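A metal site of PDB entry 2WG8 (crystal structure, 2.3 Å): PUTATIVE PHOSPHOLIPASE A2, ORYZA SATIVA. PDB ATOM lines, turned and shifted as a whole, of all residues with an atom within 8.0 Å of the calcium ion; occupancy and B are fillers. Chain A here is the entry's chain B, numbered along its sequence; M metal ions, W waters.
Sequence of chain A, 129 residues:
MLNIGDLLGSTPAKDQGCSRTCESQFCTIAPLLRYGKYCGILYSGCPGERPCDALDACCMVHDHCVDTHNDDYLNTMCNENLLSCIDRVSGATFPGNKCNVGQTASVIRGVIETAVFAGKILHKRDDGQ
SG of Cys 39 forms a disulfide with SG of Cys 59, at 2.0 Å. The side-chain carboxylate of Asp 56 sits at hydrogen-bond distance from the backbone NH of Tyr 38, at 2.8 Å.
Of the 19 residues printed, 4 come within 4 Å of the calcium ion.
The calcium ion is bound by O of Tyr 43 (2.2 Å), O of Tyr 38 (2.3 Å), O of Gly 40 (2.6 Å), water W2 (2.6 Å), OD1 of Asp 63 (2.6 Å) and OD2 of Asp 63 (2.7 Å).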
ATOM      1  N   LEU A  33     -28.597   1.732 -30.286  1.00  0.00           N
ATOM      2  CA  LEU A  33     -27.467   0.855 -30.553  1.00  0.00           C
ATOM      3  C   LEU A  33     -26.415   0.878 -29.447  1.00  0.00           C
ATOM      4  O   LEU A  33     -26.008   1.956 -29.008  1.00  0.00           O
ATOM      5  CB  LEU A  33     -26.849   1.272 -31.890  1.00  0.00           C
ATOM      6  CG  LEU A  33     -25.921   0.374 -32.704  1.00  0.00           C
ATOM      7  CD1 LEU A  33     -26.257   0.560 -34.174  1.00  0.00           C
ATOM      8  CD2 LEU A  33     -24.453   0.683 -32.446  1.00  0.00           C
ATOM      9  N   ARG A  34     -25.981  -0.308 -29.012  1.00  0.00           N
ATOM     10  CA  ARG A  34     -24.811  -0.472 -28.141  1.00  0.00           C
ATOM     11  C   ARG A  34     -24.050  -1.685 -28.663  1.00  0.00           C
ATOM     12  O   ARG A  34     -24.563  -2.800 -28.632  1.00  0.00           O
ATOM     13  CB  ARG A  34     -25.170  -0.625 -26.664  1.00  0.00           C
ATOM     14  CG  ARG A  34     -25.696   0.643 -26.064  1.00  0.00           C
ATOM     15  CD  ARG A  34     -26.070   0.507 -24.632  1.00  0.00           C
ATOM     16  NE  ARG A  34     -26.460   1.805 -24.095  1.00  0.00           N
ATOM     17  CZ  ARG A  34     -26.898   2.002 -22.857  1.00  0.00           C
ATOM     18  NH1 ARG A  34     -27.018   0.982 -22.014  1.00  0.00           N
ATOM     19  NH2 ARG A  34     -27.239   3.220 -22.468  1.00  0.00           N
ATOM     20  N   TYR A  35     -22.838  -1.434 -29.147  1.00  0.00           N
ATOM     21  CA  TYR A  35     -22.044  -2.427 -29.868  1.00  0.00           C
ATOM     22  C   TYR A  35     -20.616  -2.313 -29.365  1.00  0.00           C
ATOM     23  O   TYR A  35     -20.059  -1.214 -29.361  1.00  0.00           O
ATOM     24  CB  TYR A  35     -22.097  -2.117 -31.361  1.00  0.00           C
ATOM     25  CG  TYR A  35     -21.244  -2.985 -32.272  1.00  0.00           C
ATOM     26  CD1 TYR A  35     -21.841  -3.920 -33.111  1.00  0.00           C
ATOM     27  CD2 TYR A  35     -19.847  -2.830 -32.336  1.00  0.00           C
ATOM     28  CE1 TYR A  35     -21.070  -4.708 -33.976  1.00  0.00           C
ATOM     29  CE2 TYR A  35     -19.086  -3.610 -33.166  1.00  0.00           C
ATOM     30  CZ  TYR A  35     -19.704  -4.537 -34.004  1.00  0.00           C
ATOM     31  OH  TYR A  35     -18.950  -5.320 -34.855  1.00  0.00           O
ATOM     32  N   LYS A  37     -17.673  -1.970 -26.691  1.00  0.00           N
ATOM     33  CA  LYS A  37     -17.646  -1.050 -25.540  1.00  0.00           C
ATOM     34  C   LYS A  37     -17.872   0.413 -25.953  1.00  0.00           C
ATOM     35  O   LYS A  37     -18.128   1.260 -25.088  1.00  0.00           O
ATOM     36  CB  LYS A  37     -16.315  -1.154 -24.809  1.00  0.00           C
ATOM     37  CG  LYS A  37     -15.993  -2.541 -24.290  1.00  0.00           C
ATOM     38  CD  LYS A  37     -14.549  -2.637 -23.824  1.00  0.00           C
ATOM     39  CE  LYS A  37     -14.175  -4.080 -23.534  1.00  0.00           C
ATOM     40  NZ  LYS A  37     -12.742  -4.184 -23.196  1.00  0.00           N
ATOM     41  N   TYR A  38     -17.775   0.719 -27.253  1.00  0.00           N
ATOM     42  CA  TYR A  38     -17.746   2.114 -27.698  1.00  0.00           C
ATOM     43  C   TYR A  38     -18.830   2.540 -28.700  1.00  0.00           C
ATOM     44  O   TYR A  38     -19.168   3.721 -28.749  1.00  0.00           O
ATOM     45  CB  TYR A  38     -16.358   2.501 -28.243  1.00  0.00           C
ATOM     46  CG  TYR A  38     -15.226   2.430 -27.223  1.00  0.00           C
ATOM     47  CD1 TYR A  38     -14.438   1.265 -27.087  1.00  0.00           C
ATOM     48  CD2 TYR A  38     -14.922   3.523 -26.425  1.00  0.00           C
ATOM     49  CE1 TYR A  38     -13.401   1.210 -26.161  1.00  0.00           C
ATOM     50  CE2 TYR A  38     -13.887   3.477 -25.504  1.00  0.00           C
ATOM     51  CZ  TYR A  38     -13.130   2.319 -25.363  1.00  0.00           C
ATOM     52  OH  TYR A  38     -12.110   2.305 -24.422  1.00  0.00           O
ATOM     53  N   CYS A  39     -19.376   1.619 -29.478  1.00  0.00           N
ATOM     54  CA  CYS A  39     -20.337   2.022 -30.527  1.00  0.00           C
ATOM     55  C   CYS A  39     -21.731   2.248 -29.973  1.00  0.00           C
ATOM     56  O   CYS A  39     -22.374   1.325 -29.458  1.00  0.00           O
ATOM     57  CB  CYS A  39     -20.358   1.019 -31.699  1.00  0.00           C
ATOM     58  SG  CYS A  39     -18.793   0.879 -32.589  1.00  0.00           S
ATOM     59  N   GLY A  40     -22.187   3.482 -30.084  1.00  0.00           N
ATOM     60  CA  GLY A  40     -23.505   3.872 -29.603  1.00  0.00           C
ATOM     61  C   GLY A  40     -23.468   5.271 -29.043  1.00  0.00           C
ATOM     62  O   GLY A  40     -22.467   5.689 -28.464  1.00  0.00           O
ATOM     63  N   ILE A  41     -24.568   6.006 -29.238  1.00  0.00           N
ATOM     64  CA  ILE A  41     -24.654   7.384 -28.763  1.00  0.00           C
ATOM     65  C   ILE A  41     -24.720   7.365 -27.218  1.00  0.00           C
ATOM     66  O   ILE A  41     -25.456   6.566 -26.621  1.00  0.00           O
ATOM     67  CB  ILE A  41     -25.883   8.138 -29.406  1.00  0.00           C
ATOM     68  CG1 ILE A  41     -25.912   7.894 -30.916  1.00  0.00           C
ATOM     69  CG2 ILE A  41     -25.794   9.644 -29.122  1.00  0.00           C
ATOM     70  CD1 ILE A  41     -27.230   8.250 -31.611  1.00  0.00           C
ATOM     71  N   LEU A  42     -23.933   8.226 -26.575  1.00  0.00           N
ATOM     72  CA  LEU A  42     -23.922   8.285 -25.107  1.00  0.00           C
ATOM     73  C   LEU A  42     -23.507   6.961 -24.461  1.00  0.00           C
ATOM     74  O   LEU A  42     -23.967   6.597 -23.371  1.00  0.00           O
ATOM     75  CB  LEU A  42     -25.293   8.728 -24.558  1.00  0.00           C
ATOM     76  CG  LEU A  42     -25.702  10.182 -24.796  1.00  0.00           C
ATOM     77  CD1 LEU A  42     -27.050  10.413 -24.135  1.00  0.00           C
ATOM     78  CD2 LEU A  42     -24.651  11.137 -24.237  1.00  0.00           C
ATOM     79  N   TYR A  43     -22.654   6.224 -25.136  1.00  0.00           N
ATOM     80  CA  TYR A  43     -22.258   4.910 -24.702  1.00  0.00           C
ATOM     81  C   TYR A  43     -20.790   4.812 -25.054  1.00  0.00           C
ATOM     82  O   TYR A  43     -20.448   4.889 -26.237  1.00  0.00           O
ATOM     83  CB  TYR A  43     -23.044   3.826 -25.457  1.00  0.00           C
ATOM     84  CG  TYR A  43     -22.516   2.452 -25.173  1.00  0.00           C
ATOM     85  CD1 TYR A  43     -22.701   1.861 -23.914  1.00  0.00           C
ATOM     86  CD2 TYR A  43     -21.776   1.749 -26.123  1.00  0.00           C
ATOM     87  CE1 TYR A  43     -22.188   0.602 -23.630  1.00  0.00           C
ATOM     88  CE2 TYR A  43     -21.259   0.502 -25.860  1.00  0.00           C
ATOM     89  CZ  TYR A  43     -21.472  -0.070 -24.619  1.00  0.00           C
ATOM     90  OH  TYR A  43     -20.960  -1.320 -24.339  1.00  0.00           O
ATOM     91  N   SER A  44     -19.942   4.623 -24.041  1.00  0.00           N
ATOM     92  CA  SER A  44     -18.505   4.577 -24.256  1.00  0.00           C
ATOM     93  C   SER A  44     -17.800   3.691 -23.235  1.00  0.00           C
ATOM     94  O   SER A  44     -18.357   3.367 -22.180  1.00  0.00           O
ATOM     95  CB  SER A  44     -17.923   5.998 -24.242  1.00  0.00           C
ATOM     96  OG  SER A  44     -16.837   6.091 -25.154  1.00  0.00           O
ATOM     97  N   GLY A  45     -16.567   3.293 -23.560  1.00  0.00           N
ATOM     98  CA  GLY A  45     -15.787   2.429 -22.690  1.00  0.00           C
ATOM     99  C   GLY A  45     -15.057   3.182 -21.593  1.00  0.00           C
ATOM    100  O   GLY A  45     -14.823   4.380 -21.694  1.00  0.00           O
ATOM    101  N   ASP A  56     -15.555  -1.360 -33.333  1.00  0.00           N
ATOM    102  CA  ASP A  56     -15.524  -0.807 -31.983  1.00  0.00           C
ATOM    103  C   ASP A  56     -14.363   0.192 -31.787  1.00  0.00           C
ATOM    104  O   ASP A  56     -14.495   1.161 -31.044  1.00  0.00           O
ATOM    105  CB  ASP A  56     -15.479  -1.926 -30.936  1.00  0.00           C
ATOM    106  CG  ASP A  56     -15.998  -1.492 -29.572  1.00  0.00           C
ATOM    107  OD1 ASP A  56     -16.888  -0.619 -29.502  1.00  0.00           O
ATOM    108  OD2 ASP A  56     -15.516  -2.037 -28.552  1.00  0.00           O
ATOM    109  N   CYS A  59     -15.302   3.650 -33.335  1.00  0.00           N
ATOM    110  CA  CYS A  59     -16.157   4.322 -32.353  1.00  0.00           C
ATOM    111  C   CYS A  59     -15.376   4.849 -31.156  1.00  0.00           C
ATOM    112  O   CYS A  59     -15.690   5.916 -30.636  1.00  0.00           O
ATOM    113  CB  CYS A  59     -17.251   3.372 -31.866  1.00  0.00           C
ATOM    114  SG  CYS A  59     -18.353   2.779 -33.144  1.00  0.00           S
ATOM    115  N   MET A  60     -14.374   4.096 -30.718  1.00  0.00           N
ATOM    116  CA  MET A  60     -13.490   4.543 -29.636  1.00  0.00           C
ATOM    117  C   MET A  60     -12.800   5.860 -29.972  1.00  0.00           C
ATOM    118  O   MET A  60     -12.798   6.778 -29.148  1.00  0.00           O
ATOM    119  CB  MET A  60     -12.443   3.480 -29.313  1.00  0.00           C
ATOM    120  CG  MET A  60     -11.461   3.878 -28.191  1.00  0.00           C
ATOM    121  SD  MET A  60     -10.111   2.703 -28.110  1.00  0.00           S
ATOM    122  CE  MET A  60      -9.388   3.073 -26.501  1.00  0.00           C
ATOM    123  N   HIS A  62     -13.721   8.087 -32.374  1.00  0.00           N
ATOM    124  CA  HIS A  62     -14.766   9.101 -32.502  1.00  0.00           C
ATOM    125  C   HIS A  62     -15.225   9.634 -31.136  1.00  0.00           C
ATOM    126  O   HIS A  62     -15.356  10.848 -30.972  1.00  0.00           O
ATOM    127  CB  HIS A  62     -15.954   8.544 -33.277  1.00  0.00           C
ATOM    128  CG  HIS A  62     -17.000   9.571 -33.601  1.00  0.00           C
ATOM    129  ND1 HIS A  62     -18.189   9.661 -32.918  1.00  0.00           N
ATOM    130  CD2 HIS A  62     -17.042  10.533 -34.555  1.00  0.00           C
ATOM    131  CE1 HIS A  62     -18.916  10.649 -33.427  1.00  0.00           C
ATOM    132  NE2 HIS A  62     -18.231  11.195 -34.423  1.00  0.00           N
ATOM    133  N   ASP A  63     -15.480   8.734 -30.182  1.00  0.00           N
ATOM    134  CA  ASP A  63     -15.880   9.117 -28.808  1.00  0.00           C
ATOM    135  C   ASP A  63     -14.921  10.119 -28.176  1.00  0.00           C
ATOM    136  O   ASP A  63     -15.349  11.097 -27.561  1.00  0.00           O
ATOM    137  CB  ASP A  63     -15.948   7.879 -27.895  1.00  0.00           C
ATOM    138  CG  ASP A  63     -17.232   7.066 -28.092  1.00  0.00           C
ATOM    139  OD1 ASP A  63     -18.123   7.487 -28.863  1.00  0.00           O
ATOM    140  OD2 ASP A  63     -17.345   5.995 -27.454  1.00  0.00           O
ATOM    141  N   HIS A  64     -13.628   9.851 -28.309  1.00  0.00           N
ATOM    142  CA  HIS A  64     -12.613  10.733 -27.738  1.00  0.00           C
ATOM    143  C   HIS A  64     -12.480  12.013 -28.550  1.00  0.00           C
ATOM    144  O   HIS A  64     -12.315  13.101 -27.980  1.00  0.00           O
ATOM    145  CB  HIS A  64     -11.278  10.007 -27.659  1.00  0.00           C
ATOM    146  CG  HIS A  64     -11.259   8.921 -26.626  1.00  0.00           C
ATOM    147  ND1 HIS A  64     -11.198   9.197 -25.272  1.00  0.00           N
ATOM    148  CD2 HIS A  64     -11.306   7.579 -26.735  1.00  0.00           C
ATOM    149  CE1 HIS A  64     -11.202   8.065 -24.601  1.00  0.00           C
ATOM    150  NE2 HIS A  64     -11.266   7.062 -25.460  1.00  0.00           N
ATOM    151  N   TYR A  73     -20.557  16.786 -31.435  1.00  0.00           N
ATOM    152  CA  TYR A  73     -20.929  15.649 -32.282  1.00  0.00           C
ATOM    153  C   TYR A  73     -20.967  16.005 -33.761  1.00  0.00           C
ATOM    154  O   TYR A  73     -20.918  15.114 -34.618  1.00  0.00           O
ATOM    155  CB  TYR A  73     -22.304  15.116 -31.904  1.00  0.00           C
ATOM    156  CG  TYR A  73     -22.385  14.530 -30.519  1.00  0.00           C
ATOM    157  CD1 TYR A  73     -22.165  13.174 -30.302  1.00  0.00           C
ATOM    158  CD2 TYR A  73     -22.723  15.340 -29.429  1.00  0.00           C
ATOM    159  CE1 TYR A  73     -22.249  12.633 -29.021  1.00  0.00           C
ATOM    160  CE2 TYR A  73     -22.807  14.812 -28.145  1.00  0.00           C
ATOM    161  CZ  TYR A  73     -22.572  13.460 -27.948  1.00  0.00           C
ATOM    162  OH  TYR A  73     -22.661  12.935 -26.677  1.00  0.00           O
HETATM  163 CA    CA M   1     -19.921   5.772 -28.187  1.00  0.00          CA
HETATM  164  O   HOH W   1     -19.856   6.203 -31.410  1.00  0.00           O
HETATM  165  O   HOH W   2     -20.676   7.988 -27.137  1.00  0.00           O
